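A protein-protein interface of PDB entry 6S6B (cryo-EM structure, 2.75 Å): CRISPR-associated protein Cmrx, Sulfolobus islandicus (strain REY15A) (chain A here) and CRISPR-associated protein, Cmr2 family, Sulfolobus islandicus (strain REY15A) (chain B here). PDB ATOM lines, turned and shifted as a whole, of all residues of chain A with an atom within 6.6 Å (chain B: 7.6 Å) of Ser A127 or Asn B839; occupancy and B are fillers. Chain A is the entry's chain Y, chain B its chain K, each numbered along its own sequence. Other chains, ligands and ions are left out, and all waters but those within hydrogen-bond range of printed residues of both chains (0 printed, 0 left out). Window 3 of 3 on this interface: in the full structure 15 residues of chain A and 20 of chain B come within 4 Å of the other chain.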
ATOM      1  N   PRO A  11     -33.317   4.920  11.073  1.00  0.00           N
ATOM      2  CA  PRO A  11     -33.113   5.067   9.632  1.00  0.00           C
ATOM      3  C   PRO A  11     -32.697   6.492   9.281  1.00  0.00           C
ATOM      4  O   PRO A  11     -32.641   7.381  10.132  1.00  0.00           O
ATOM      5  CB  PRO A  11     -34.497   4.745   9.064  1.00  0.00           C
ATOM      6  CG  PRO A  11     -35.425   5.278  10.095  1.00  0.00           C
ATOM      7  CD  PRO A  11     -34.722   5.172  11.437  1.00  0.00           C
ATOM      8  N   ILE A  12     -32.403   6.693   7.995  1.00  0.00           N
ATOM      9  CA  ILE A  12     -32.060   8.025   7.506  1.00  0.00           C
ATOM     10  C   ILE A  12     -33.272   8.930   7.366  1.00  0.00           C
ATOM     11  O   ILE A  12     -33.111  10.130   7.115  1.00  0.00           O
ATOM     12  CB  ILE A  12     -31.344   7.952   6.142  1.00  0.00           C
ATOM     13  CG1 ILE A  12     -32.357   7.671   5.028  1.00  0.00           C
ATOM     14  CG2 ILE A  12     -30.243   6.901   6.172  1.00  0.00           C
ATOM     15  CD1 ILE A  12     -31.840   7.942   3.632  1.00  0.00           C
ATOM     16  N   PRO A 125     -31.810  -2.710   0.755  1.00  0.00           N
ATOM     17  CA  PRO A 125     -30.705  -2.494   1.696  1.00  0.00           C
ATOM     18  C   PRO A 125     -30.282  -1.034   1.722  1.00  0.00           C
ATOM     19  O   PRO A 125     -30.247  -0.360   0.691  1.00  0.00           O
ATOM     20  CB  PRO A 125     -29.594  -3.398   1.153  1.00  0.00           C
ATOM     21  CG  PRO A 125     -29.923  -3.574  -0.283  1.00  0.00           C
ATOM     22  CD  PRO A 125     -31.418  -3.584  -0.361  1.00  0.00           C
ATOM     23  N   VAL A 126     -29.958  -0.548   2.921  1.00  0.00           N
ATOM     24  CA  VAL A 126     -29.649   0.863   3.125  1.00  0.00           C
ATOM     25  C   VAL A 126     -28.990   1.025   4.487  1.00  0.00           C
ATOM     26  O   VAL A 126     -29.252   0.255   5.417  1.00  0.00           O
ATOM     27  CB  VAL A 126     -30.931   1.724   2.987  1.00  0.00           C
ATOM     28  CG1 VAL A 126     -31.976   1.264   3.980  1.00  0.00           C
ATOM     29  CG2 VAL A 126     -30.620   3.206   3.162  1.00  0.00           C
ATOM     30  N   SER A 127     -28.122   2.028   4.601  1.00  0.00           N
ATOM     31  CA  SER A 127     -27.425   2.326   5.843  1.00  0.00           C
ATOM     32  C   SER A 127     -27.261   3.838   5.946  1.00  0.00           C
ATOM     33  O   SER A 127     -27.926   4.600   5.240  1.00  0.00           O
ATOM     34  CB  SER A 127     -26.086   1.582   5.912  1.00  0.00           C
ATOM     35  OG  SER A 127     -26.291   0.191   6.090  1.00  0.00           O
ATOM     36  N   ILE A 128     -26.369   4.278   6.827  1.00  0.00           N
ATOM     37  CA  ILE A 128     -26.198   5.695   7.120  1.00  0.00           C
ATOM     38  C   ILE A 128     -24.777   6.119   6.766  1.00  0.00           C
ATOM     39  O   ILE A 128     -23.809   5.413   7.062  1.00  0.00           O
ATOM     40  CB  ILE A 128     -26.522   6.024   8.591  1.00  0.00           C
ATOM     41  CG1 ILE A 128     -28.000   5.749   8.890  1.00  0.00           C
ATOM     42  CG2 ILE A 128     -26.206   7.479   8.897  1.00  0.00           C
ATOM     43  CD1 ILE A 128     -28.289   4.348   9.392  1.00  0.00           C
ATOM     44  N   SER A 129     -24.672   7.272   6.116  1.00  0.00           N
ATOM     45  CA  SER A 129     -23.422   7.909   5.715  1.00  0.00           C
ATOM     46  C   SER A 129     -23.675   9.413   5.717  1.00  0.00           C
ATOM     47  O   SER A 129     -24.606   9.887   6.376  1.00  0.00           O
ATOM     48  CB  SER A 129     -22.958   7.363   4.354  1.00  0.00           C
ATOM     49  OG  SER A 129     -21.692   7.887   4.000  1.00  0.00           O
ATOM     50  N   ILE A 133     -26.448  13.474   7.161  1.00  0.00           N
ATOM     51  CA  ILE A 133     -27.431  12.418   7.385  1.00  0.00           C
ATOM     52  C   ILE A 133     -27.233  11.757   8.747  1.00  0.00           C
ATOM     53  O   ILE A 133     -28.140  11.081   9.247  1.00  0.00           O
ATOM     54  CB  ILE A 133     -27.371  11.412   6.217  1.00  0.00           C
ATOM     55  CG1 ILE A 133     -27.753  12.108   4.910  1.00  0.00           C
ATOM     56  CG2 ILE A 133     -28.302  10.233   6.426  1.00  0.00           C
ATOM     57  CD1 ILE A 133     -29.179  12.627   4.885  1.00  0.00           C
ATOM     58  N   ILE A 163     -23.785   4.980  14.491  1.00  0.00           N
ATOM     59  CA  ILE A 163     -24.934   5.134  13.604  1.00  0.00           C
ATOM     60  C   ILE A 163     -24.642   4.495  12.255  1.00  0.00           C
ATOM     61  O   ILE A 163     -25.493   3.809  11.682  1.00  0.00           O
ATOM     62  CB  ILE A 163     -25.316   6.620  13.446  1.00  0.00           C
ATOM     63  CG1 ILE A 163     -25.736   7.227  14.784  1.00  0.00           C
ATOM     64  CG2 ILE A 163     -26.443   6.778  12.441  1.00  0.00           C
ATOM     65  CD1 ILE A 163     -24.616   7.908  15.518  1.00  0.00           C
ATOM     66  N   LYS A 164     -23.432   4.697  11.740  1.00  0.00           N
ATOM     67  CA  LYS A 164     -23.007   4.109  10.480  1.00  0.00           C
ATOM     68  C   LYS A 164     -22.320   2.762  10.657  1.00  0.00           C
ATOM     69  O   LYS A 164     -21.980   2.123   9.656  1.00  0.00           O
ATOM     70  CB  LYS A 164     -22.070   5.074   9.748  1.00  0.00           C
ATOM     71  CG  LYS A 164     -22.586   6.505   9.716  1.00  0.00           C
ATOM     72  CD  LYS A 164     -21.656   7.419   8.942  1.00  0.00           C
ATOM     73  CE  LYS A 164     -20.310   7.543   9.629  1.00  0.00           C
ATOM     74  NZ  LYS A 164     -20.414   8.233  10.941  1.00  0.00           N
ATOM     75  N   PHE A 167     -26.447   0.300  13.082  1.00  0.00           N
ATOM     76  CA  PHE A 167     -27.845   0.310  12.658  1.00  0.00           C
ATOM     77  C   PHE A 167     -27.900   0.309  11.136  1.00  0.00           C
ATOM     78  O   PHE A 167     -27.746   1.351  10.495  1.00  0.00           O
ATOM     79  CB  PHE A 167     -28.565   1.520  13.242  1.00  0.00           C
ATOM     80  CG  PHE A 167     -28.358   1.690  14.720  1.00  0.00           C
ATOM     81  CD1 PHE A 167     -27.313   2.466  15.199  1.00  0.00           C
ATOM     82  CD2 PHE A 167     -29.194   1.073  15.633  1.00  0.00           C
ATOM     83  CE1 PHE A 167     -27.112   2.626  16.557  1.00  0.00           C
ATOM     84  CE2 PHE A 167     -28.997   1.232  16.993  1.00  0.00           C
ATOM     85  CZ  PHE A 167     -27.953   2.008  17.453  1.00  0.00           C
ATOM     86  N   SER A 168     -28.115  -0.868  10.554  1.00  0.00           N
ATOM     87  CA  SER A 168     -28.334  -1.021   9.122  1.00  0.00           C
ATOM     88  C   SER A 168     -29.695  -1.665   8.916  1.00  0.00           C
ATOM     89  O   SER A 168     -29.917  -2.803   9.342  1.00  0.00           O
ATOM     90  CB  SER A 168     -27.226  -1.856   8.477  1.00  0.00           C
ATOM     91  OG  SER A 168     -27.229  -3.185   8.967  1.00  0.00           O
ATOM     92  N   TYR A 169     -30.598  -0.942   8.268  1.00  0.00           N
ATOM     93  CA  TYR A 169     -31.987  -1.348   8.112  1.00  0.00           C
ATOM     94  C   TYR A 169     -32.273  -1.711   6.658  1.00  0.00           C
ATOM     95  O   TYR A 169     -31.415  -1.592   5.778  1.00  0.00           O
ATOM     96  CB  TYR A 169     -32.922  -0.241   8.603  1.00  0.00           C
ATOM     97  CG  TYR A 169     -32.809   1.062   7.848  1.00  0.00           C
ATOM     98  CD1 TYR A 169     -31.660   1.837   7.920  1.00  0.00           C
ATOM     99  CD2 TYR A 169     -33.861   1.525   7.077  1.00  0.00           C
ATOM    100  CE1 TYR A 169     -31.558   3.027   7.232  1.00  0.00           C
ATOM    101  CE2 TYR A 169     -33.775   2.716   6.392  1.00  0.00           C
ATOM    102  CZ  TYR A 169     -32.621   3.464   6.471  1.00  0.00           C
ATOM    103  OH  TYR A 169     -32.533   4.649   5.782  1.00  0.00           O
ATOM    104  N   ASN B 103     -13.489  -7.808   7.716  1.00  0.00           N
ATOM    105  CA  ASN B 103     -13.093  -8.321   6.416  1.00  0.00           C
ATOM    106  C   ASN B 103     -11.605  -8.658   6.425  1.00  0.00           C
ATOM    107  O   ASN B 103     -10.844  -8.201   7.280  1.00  0.00           O
ATOM    108  CB  ASN B 103     -13.404  -7.299   5.325  1.00  0.00           C
ATOM    109  CG  ASN B 103     -13.437  -7.912   3.944  1.00  0.00           C
ATOM    110  OD1 ASN B 103     -12.486  -8.560   3.518  1.00  0.00           O
ATOM    111  ND2 ASN B 103     -14.538  -7.713   3.237  1.00  0.00           N
ATOM    112  N   LEU B 106     -10.095  -5.743   3.370  1.00  0.00           N
ATOM    113  CA  LEU B 106     -10.221  -4.488   4.087  1.00  0.00           C
ATOM    114  C   LEU B 106     -10.312  -4.724   5.582  1.00  0.00           C
ATOM    115  O   LEU B 106     -10.588  -5.828   6.051  1.00  0.00           O
ATOM    116  CB  LEU B 106     -11.441  -3.700   3.624  1.00  0.00           C
ATOM    117  CG  LEU B 106     -11.196  -2.994   2.310  1.00  0.00           C
ATOM    118  CD1 LEU B 106     -12.459  -2.357   1.825  1.00  0.00           C
ATOM    119  CD2 LEU B 106     -10.127  -1.953   2.550  1.00  0.00           C
ATOM    120  N   ILE B 109     -14.070  -2.274   7.379  1.00  0.00           N
ATOM    121  CA  ILE B 109     -15.412  -2.829   7.282  1.00  0.00           C
ATOM    122  C   ILE B 109     -15.536  -3.959   8.288  1.00  0.00           C
ATOM    123  O   ILE B 109     -14.676  -4.844   8.349  1.00  0.00           O
ATOM    124  CB  ILE B 109     -15.723  -3.338   5.863  1.00  0.00           C
ATOM    125  CG1 ILE B 109     -15.169  -2.370   4.825  1.00  0.00           C
ATOM    126  CG2 ILE B 109     -17.218  -3.505   5.682  1.00  0.00           C
ATOM    127  CD1 ILE B 109     -15.529  -2.748   3.431  1.00  0.00           C
ATOM    128  N   GLN B 110     -16.601  -3.924   9.084  1.00  0.00           N
ATOM    129  CA  GLN B 110     -16.855  -4.976  10.054  1.00  0.00           C
ATOM    130  C   GLN B 110     -18.349  -5.238  10.123  1.00  0.00           C
ATOM    131  O   GLN B 110     -19.168  -4.383   9.780  1.00  0.00           O
ATOM    132  CB  GLN B 110     -16.343  -4.615  11.452  1.00  0.00           C
ATOM    133  CG  GLN B 110     -15.029  -3.868  11.490  1.00  0.00           C
ATOM    134  CD  GLN B 110     -14.920  -2.977  12.702  1.00  0.00           C
ATOM    135  OE1 GLN B 110     -15.513  -3.252  13.742  1.00  0.00           O
ATOM    136  NE2 GLN B 110     -14.167  -1.895  12.572  1.00  0.00           N
ATOM    137  N   ARG B 111     -18.689  -6.440  10.569  1.00  0.00           N
ATOM    138  CA  ARG B 111     -20.034  -6.767  11.003  1.00  0.00           C
ATOM    139  C   ARG B 111     -19.990  -6.965  12.507  1.00  0.00           C
ATOM    140  O   ARG B 111     -18.919  -6.977  13.119  1.00  0.00           O
ATOM    141  CB  ARG B 111     -20.570  -8.019  10.306  1.00  0.00           C
ATOM    142  CG  ARG B 111     -20.624  -7.900   8.809  1.00  0.00           C
ATOM    143  CD  ARG B 111     -21.380  -6.660   8.395  1.00  0.00           C
ATOM    144  NE  ARG B 111     -22.788  -6.735   8.766  1.00  0.00           N
ATOM    145  CZ  ARG B 111     -23.757  -6.096   8.122  1.00  0.00           C
ATOM    146  NH1 ARG B 111     -23.469  -5.338   7.074  1.00  0.00           N
ATOM    147  NH2 ARG B 111     -25.014  -6.216   8.522  1.00  0.00           N
ATOM    148  N   ALA B 825     -17.830  -6.620  -5.316  1.00  0.00           N
ATOM    149  CA  ALA B 825     -17.317  -5.885  -4.171  1.00  0.00           C
ATOM    150  C   ALA B 825     -18.171  -6.060  -2.928  1.00  0.00           C
ATOM    151  O   ALA B 825     -17.952  -5.353  -1.942  1.00  0.00           O
ATOM    152  CB  ALA B 825     -17.200  -4.399  -4.510  1.00  0.00           C
ATOM    153  N   GLY B 826     -19.137  -6.971  -2.948  1.00  0.00           N
ATOM    154  CA  GLY B 826     -19.944  -7.237  -1.776  1.00  0.00           C
ATOM    155  C   GLY B 826     -21.131  -6.313  -1.633  1.00  0.00           C
ATOM    156  O   GLY B 826     -22.147  -6.685  -1.046  1.00  0.00           O
ATOM    157  N   PHE B 827     -21.012  -5.097  -2.152  1.00  0.00           N
ATOM    158  CA  PHE B 827     -22.135  -4.176  -2.151  1.00  0.00           C
ATOM    159  C   PHE B 827     -23.174  -4.625  -3.165  1.00  0.00           C
ATOM    160  O   PHE B 827     -22.848  -5.161  -4.225  1.00  0.00           O
ATOM    161  CB  PHE B 827     -21.658  -2.763  -2.475  1.00  0.00           C
ATOM    162  CG  PHE B 827     -22.760  -1.809  -2.824  1.00  0.00           C
ATOM    163  CD1 PHE B 827     -23.452  -1.144  -1.834  1.00  0.00           C
ATOM    164  CD2 PHE B 827     -23.087  -1.560  -4.143  1.00  0.00           C
ATOM    165  CE1 PHE B 827     -24.460  -0.260  -2.153  1.00  0.00           C
ATOM    166  CE2 PHE B 827     -24.092  -0.680  -4.465  1.00  0.00           C
ATOM    167  CZ  PHE B 827     -24.778  -0.028  -3.471  1.00  0.00           C
ATOM    168  N   GLY B 828     -24.436  -4.398  -2.840  1.00  0.00           N
ATOM    169  CA  GLY B 828     -25.487  -4.796  -3.751  1.00  0.00           C
ATOM    170  C   GLY B 828     -26.851  -4.574  -3.147  1.00  0.00           C
ATOM    171  O   GLY B 828     -27.007  -4.347  -1.946  1.00  0.00           O
ATOM    172  N   CYS B 836     -27.459 -12.486   0.519  1.00  0.00           N
ATOM    173  CA  CYS B 836     -27.575 -11.050   0.317  1.00  0.00           C
ATOM    174  C   CYS B 836     -26.195 -10.408   0.234  1.00  0.00           C
ATOM    175  O   CYS B 836     -25.177 -11.011   0.574  1.00  0.00           O
ATOM    176  CB  CYS B 836     -28.383 -10.409   1.443  1.00  0.00           C
ATOM    177  SG  CYS B 836     -30.096 -10.911   1.527  1.00  0.00           S
ATOM    178  N   LEU B 837     -26.178  -9.155  -0.211  1.00  0.00           N
ATOM    179  CA  LEU B 837     -24.946  -8.405  -0.428  1.00  0.00           C
ATOM    180  C   LEU B 837     -24.939  -7.216   0.524  1.00  0.00           C
ATOM    181  O   LEU B 837     -25.666  -6.242   0.309  1.00  0.00           O
ATOM    182  CB  LEU B 837     -24.837  -7.944  -1.881  1.00  0.00           C
ATOM    183  CG  LEU B 837     -24.338  -8.942  -2.929  1.00  0.00           C
ATOM    184  CD1 LEU B 837     -22.961  -9.466  -2.559  1.00  0.00           C
ATOM    185  CD2 LEU B 837     -25.316 -10.080  -3.150  1.00  0.00           C
ATOM    186  N   GLU B 838     -24.110  -7.285   1.563  1.00  0.00           N
ATOM    187  CA  GLU B 838     -24.126  -6.303   2.648  1.00  0.00           C
ATOM    188  C   GLU B 838     -22.784  -5.587   2.722  1.00  0.00           C
ATOM    189  O   GLU B 838     -21.929  -5.949   3.531  1.00  0.00           O
ATOM    190  CB  GLU B 838     -24.455  -6.992   3.975  1.00  0.00           C
ATOM    191  CG  GLU B 838     -25.930  -7.262   4.198  1.00  0.00           C
ATOM    192  CD  GLU B 838     -26.351  -8.623   3.693  1.00  0.00           C
ATOM    193  OE1 GLU B 838     -25.594  -9.225   2.905  1.00  0.00           O
ATOM    194  OE2 GLU B 838     -27.435  -9.095   4.093  1.00  0.00           O
ATOM    195  N   ASN B 839     -22.626  -4.551   1.902  1.00  0.00           N
ATOM    196  CA  ASN B 839     -21.490  -3.627   1.950  1.00  0.00           C
ATOM    197  C   ASN B 839     -20.168  -4.360   2.166  1.00  0.00           C
ATOM    198  O   ASN B 839     -19.466  -4.167   3.159  1.00  0.00           O
ATOM    199  CB  ASN B 839     -21.708  -2.567   3.022  1.00  0.00           C
ATOM    200  CG  ASN B 839     -23.088  -1.963   2.959  1.00  0.00           C
ATOM    201  OD1 ASN B 839     -23.762  -1.815   3.977  1.00  0.00           O
ATOM    202  ND2 ASN B 839     -23.522  -1.615   1.754  1.00  0.00           N
ATOM    203  N   GLY B 840     -19.841  -5.223   1.212  1.00  0.00           N
ATOM    204  CA  GLY B 840     -18.611  -5.979   1.297  1.00  0.00           C
ATOM    205  C   GLY B 840     -18.701  -7.208   2.166  1.00  0.00           C
ATOM    206  O   GLY B 840     -17.689  -7.639   2.722  1.00  0.00           O
ATOM    207  N   PHE B 841     -19.891  -7.788   2.302  1.00  0.00           N
ATOM    208  CA  PHE B 841     -20.065  -8.970   3.139  1.00  0.00           C
ATOM    209  C   PHE B 841     -21.278  -9.730   2.610  1.00  0.00           C
ATOM    210  O   PHE B 841     -22.415  -9.340   2.881  1.00  0.00           O
ATOM    211  CB  PHE B 841     -20.248  -8.589   4.595  1.00  0.00           C
ATOM    212  CG  PHE B 841     -18.978  -8.550   5.373  1.00  0.00           C
ATOM    213  CD1 PHE B 841     -18.352  -9.718   5.749  1.00  0.00           C
ATOM    214  CD2 PHE B 841     -18.416  -7.345   5.743  1.00  0.00           C
ATOM    215  CE1 PHE B 841     -17.186  -9.687   6.467  1.00  0.00           C
ATOM    216  CE2 PHE B 841     -17.247  -7.306   6.462  1.00  0.00           C
ATOM    217  CZ  PHE B 841     -16.632  -8.479   6.827  1.00  0.00           C
ATOM    218  N   VAL B 842     -21.028 -10.803   1.863  1.00  0.00           N
ATOM    219  CA  VAL B 842     -22.119 -11.671   1.450  1.00  0.00           C
ATOM    220  C   VAL B 842     -22.642 -12.411   2.674  1.00  0.00           C
ATOM    221  O   VAL B 842     -21.868 -12.953   3.472  1.00  0.00           O
ATOM    222  CB  VAL B 842     -21.663 -12.630   0.339  1.00  0.00           C
ATOM    223  CG1 VAL B 842     -20.452 -13.430   0.772  1.00  0.00           C
ATOM    224  CG2 VAL B 842     -22.796 -13.552  -0.062  1.00  0.00           C
ATOM    225  N   TYR B 848     -22.261 -14.136   8.019  1.00  0.00           N
ATOM    226  CA  TYR B 848     -21.565 -13.128   7.237  1.00  0.00           C
ATOM    227  C   TYR B 848     -20.256 -13.689   6.707  1.00  0.00           C
ATOM    228  O   TYR B 848     -19.470 -14.271   7.461  1.00  0.00           O
ATOM    229  CB  TYR B 848     -21.303 -11.880   8.075  1.00  0.00           C
ATOM    230  CG  TYR B 848     -22.495 -10.969   8.163  1.00  0.00           C
ATOM    231  CD1 TYR B 848     -22.853 -10.168   7.094  1.00  0.00           C
ATOM    232  CD2 TYR B 848     -23.266 -10.915   9.310  1.00  0.00           C
ATOM    233  CE1 TYR B 848     -23.943  -9.336   7.164  1.00  0.00           C
ATOM    234  CE2 TYR B 848     -24.359 -10.084   9.390  1.00  0.00           C
ATOM    235  CZ  TYR B 848     -24.692  -9.296   8.314  1.00  0.00           C
ATOM    236  OH  TYR B 848     -25.783  -8.463   8.383  1.00  0.00           O
ATOM    237  N   SER B 851     -16.115 -10.739   1.136  1.00  0.00           N
ATOM    238  CA  SER B 851     -16.008 -10.714  -0.315  1.00  0.00           C
ATOM    239  C   SER B 851     -14.701 -10.020  -0.689  1.00  0.00           C
ATOM    240  O   SER B 851     -13.839  -9.781   0.159  1.00  0.00           O
ATOM    241  CB  SER B 851     -17.216 -10.021  -0.941  1.00  0.00           C
ATOM    242  OG  SER B 851     -17.214  -8.640  -0.639  1.00  0.00           O
ATOM    243  N   PRO B 853     -13.700  -6.681  -1.926  1.00  0.00           N
ATOM    244  CA  PRO B 853     -14.094  -5.318  -2.299  1.00  0.00           C
ATOM    245  C   PRO B 853     -12.983  -4.557  -3.000  1.00  0.00           C
ATOM    246  O   PRO B 853     -13.238  -3.746  -3.894  1.00  0.00           O
ATOM    247  CB  PRO B 853     -14.445  -4.683  -0.952  1.00  0.00           C
ATOM    248  CG  PRO B 853     -13.560  -5.383   0.015  1.00  0.00           C
ATOM    249  CD  PRO B 853     -13.367  -6.786  -0.496  1.00  0.00           C
ATOM    250  N   VAL B 926     -12.098   0.599  -2.257  1.00  0.00           N
ATOM    251  CA  VAL B 926     -12.919   0.773  -1.071  1.00  0.00           C
ATOM    252  C   VAL B 926     -11.983   0.932   0.115  1.00  0.00           C
ATOM    253  O   VAL B 926     -11.118   0.082   0.343  1.00  0.00           O
ATOM    254  CB  VAL B 926     -13.880  -0.403  -0.848  1.00  0.00           C
ATOM    255  CG1 VAL B 926     -14.823  -0.095   0.288  1.00  0.00           C
ATOM    256  CG2 VAL B 926     -14.664  -0.705  -2.111  1.00  0.00           C
ATOM    257  N   SER B 928     -13.675   2.530   2.996  1.00  0.00           N
ATOM    258  CA  SER B 928     -14.707   2.795   3.983  1.00  0.00           C
ATOM    259  C   SER B 928     -16.031   2.356   3.384  1.00  0.00           C
ATOM    260  O   SER B 928     -16.163   2.253   2.162  1.00  0.00           O
ATOM    261  CB  SER B 928     -14.756   4.277   4.370  1.00  0.00           C
ATOM    262  OG  SER B 928     -15.149   5.073   3.268  1.00  0.00           O
ATOM    263  N   VAL B 929     -17.009   2.101   4.253  1.00  0.00           N
ATOM    264  CA  VAL B 929     -18.284   1.565   3.795  1.00  0.00           C
ATOM    265  C   VAL B 929     -19.002   2.545   2.875  1.00  0.00           C
ATOM    266  O   VAL B 929     -19.861   2.142   2.086  1.00  0.00           O
ATOM    267  CB  VAL B 929     -19.140   1.185   5.020  1.00  0.00           C
ATOM    268  CG1 VAL B 929     -20.450   0.543   4.597  1.00  0.00           C
ATOM    269  CG2 VAL B 929     -18.353   0.267   5.938  1.00  0.00           C
ATOM    270  N   SER B 930     -18.646   3.824   2.930  1.00  0.00           N
ATOM    271  CA  SER B 930     -19.223   4.821   2.037  1.00  0.00           C
ATOM    272  C   SER B 930     -18.619   4.788   0.641  1.00  0.00           C
ATOM    273  O   SER B 930     -19.077   5.531  -0.231  1.00  0.00           O
ATOM    274  CB  SER B 930     -19.055   6.216   2.639  1.00  0.00           C
ATOM    275  OG  SER B 930     -17.696   6.480   2.935  1.00  0.00           O
ATOM    276  N   PHE B 932     -18.777   2.266  -1.416  1.00  0.00           N
ATOM    277  CA  PHE B 932     -19.419   1.274  -2.268  1.00  0.00           C
ATOM    278  C   PHE B 932     -20.382   1.907  -3.260  1.00  0.00           C
ATOM    279  O   PHE B 932     -20.385   1.543  -4.440  1.00  0.00           O
ATOM    280  CB  PHE B 932     -20.149   0.247  -1.412  1.00  0.00           C
ATOM    281  CG  PHE B 932     -19.236  -0.663  -0.660  1.00  0.00           C
ATOM    282  CD1 PHE B 932     -18.641  -1.734  -1.289  1.00  0.00           C
ATOM    283  CD2 PHE B 932     -18.974  -0.453   0.677  1.00  0.00           C
ATOM    284  CE1 PHE B 932     -17.803  -2.570  -0.605  1.00  0.00           C
ATOM    285  CE2 PHE B 932     -18.135  -1.291   1.366  1.00  0.00           C
ATOM    286  CZ  PHE B 932     -17.551  -2.351   0.721  1.00  0.00           C
ATOM    287  N   ASN B 933     -21.198   2.854  -2.806  1.00  0.00           N
ATOM    288  CA  ASN B 933     -22.269   3.409  -3.625  1.00  0.00           C
ATOM    289  C   ASN B 933     -21.776   4.233  -4.808  1.00  0.00           C
ATOM    290  O   ASN B 933     -22.613   4.779  -5.531  1.00  0.00           O
ATOM    291  CB  ASN B 933     -23.198   4.251  -2.752  1.00  0.00           C
ATOM    292  CG  ASN B 933     -22.464   5.341  -2.001  1.00  0.00           C
ATOM    293  OD1 ASN B 933     -21.259   5.527  -2.173  1.00  0.00           O
ATOM    294  ND2 ASN B 933     -23.187   6.071  -1.162  1.00  0.00           N
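The backbone carbonyl oxygen (O) of Ser B930 lies close to the side-chain amide oxygen (OD1) of Asn B933 (2.9 Å). The guanidinium group of Arg B111 lies close to the side-chain hydroxyl of Tyr B848, at 3.5 Å. The side-chain hydroxyl of Ser B928 is in hydrogen-bond range of the side-chain hydroxyl of Ser B930.
Gly B828 touches Pro A125 (O to CG, 3.4 Å). OD1 of Asn B839 touches OG of Ser A127, at 3.9 Å. Ser A129 touches Ser B930 (OG to CB, 3.4 Å). OG of Ser A168 touches NH2 of Arg B111 (3.8 Å).
Printed residues of chain A within 4 Å of Gly B828: Pro A125. Glu B838 touches none of the printed residues of chain A. Val B842 touches none of the printed residues of chain A. Of the printed residues of chain A, Ser B930 touches Ser A129. The nearest printed residue of chain A that does not touch Gly B828 is Val A126 (6.8 Å).
Among the printed residues, 4 pairs touch across the chains. Among the printed residues, no Asp or Glu carboxylate lies within 4 Å of a Lys or Arg side-chain nitrogen of the other chain.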
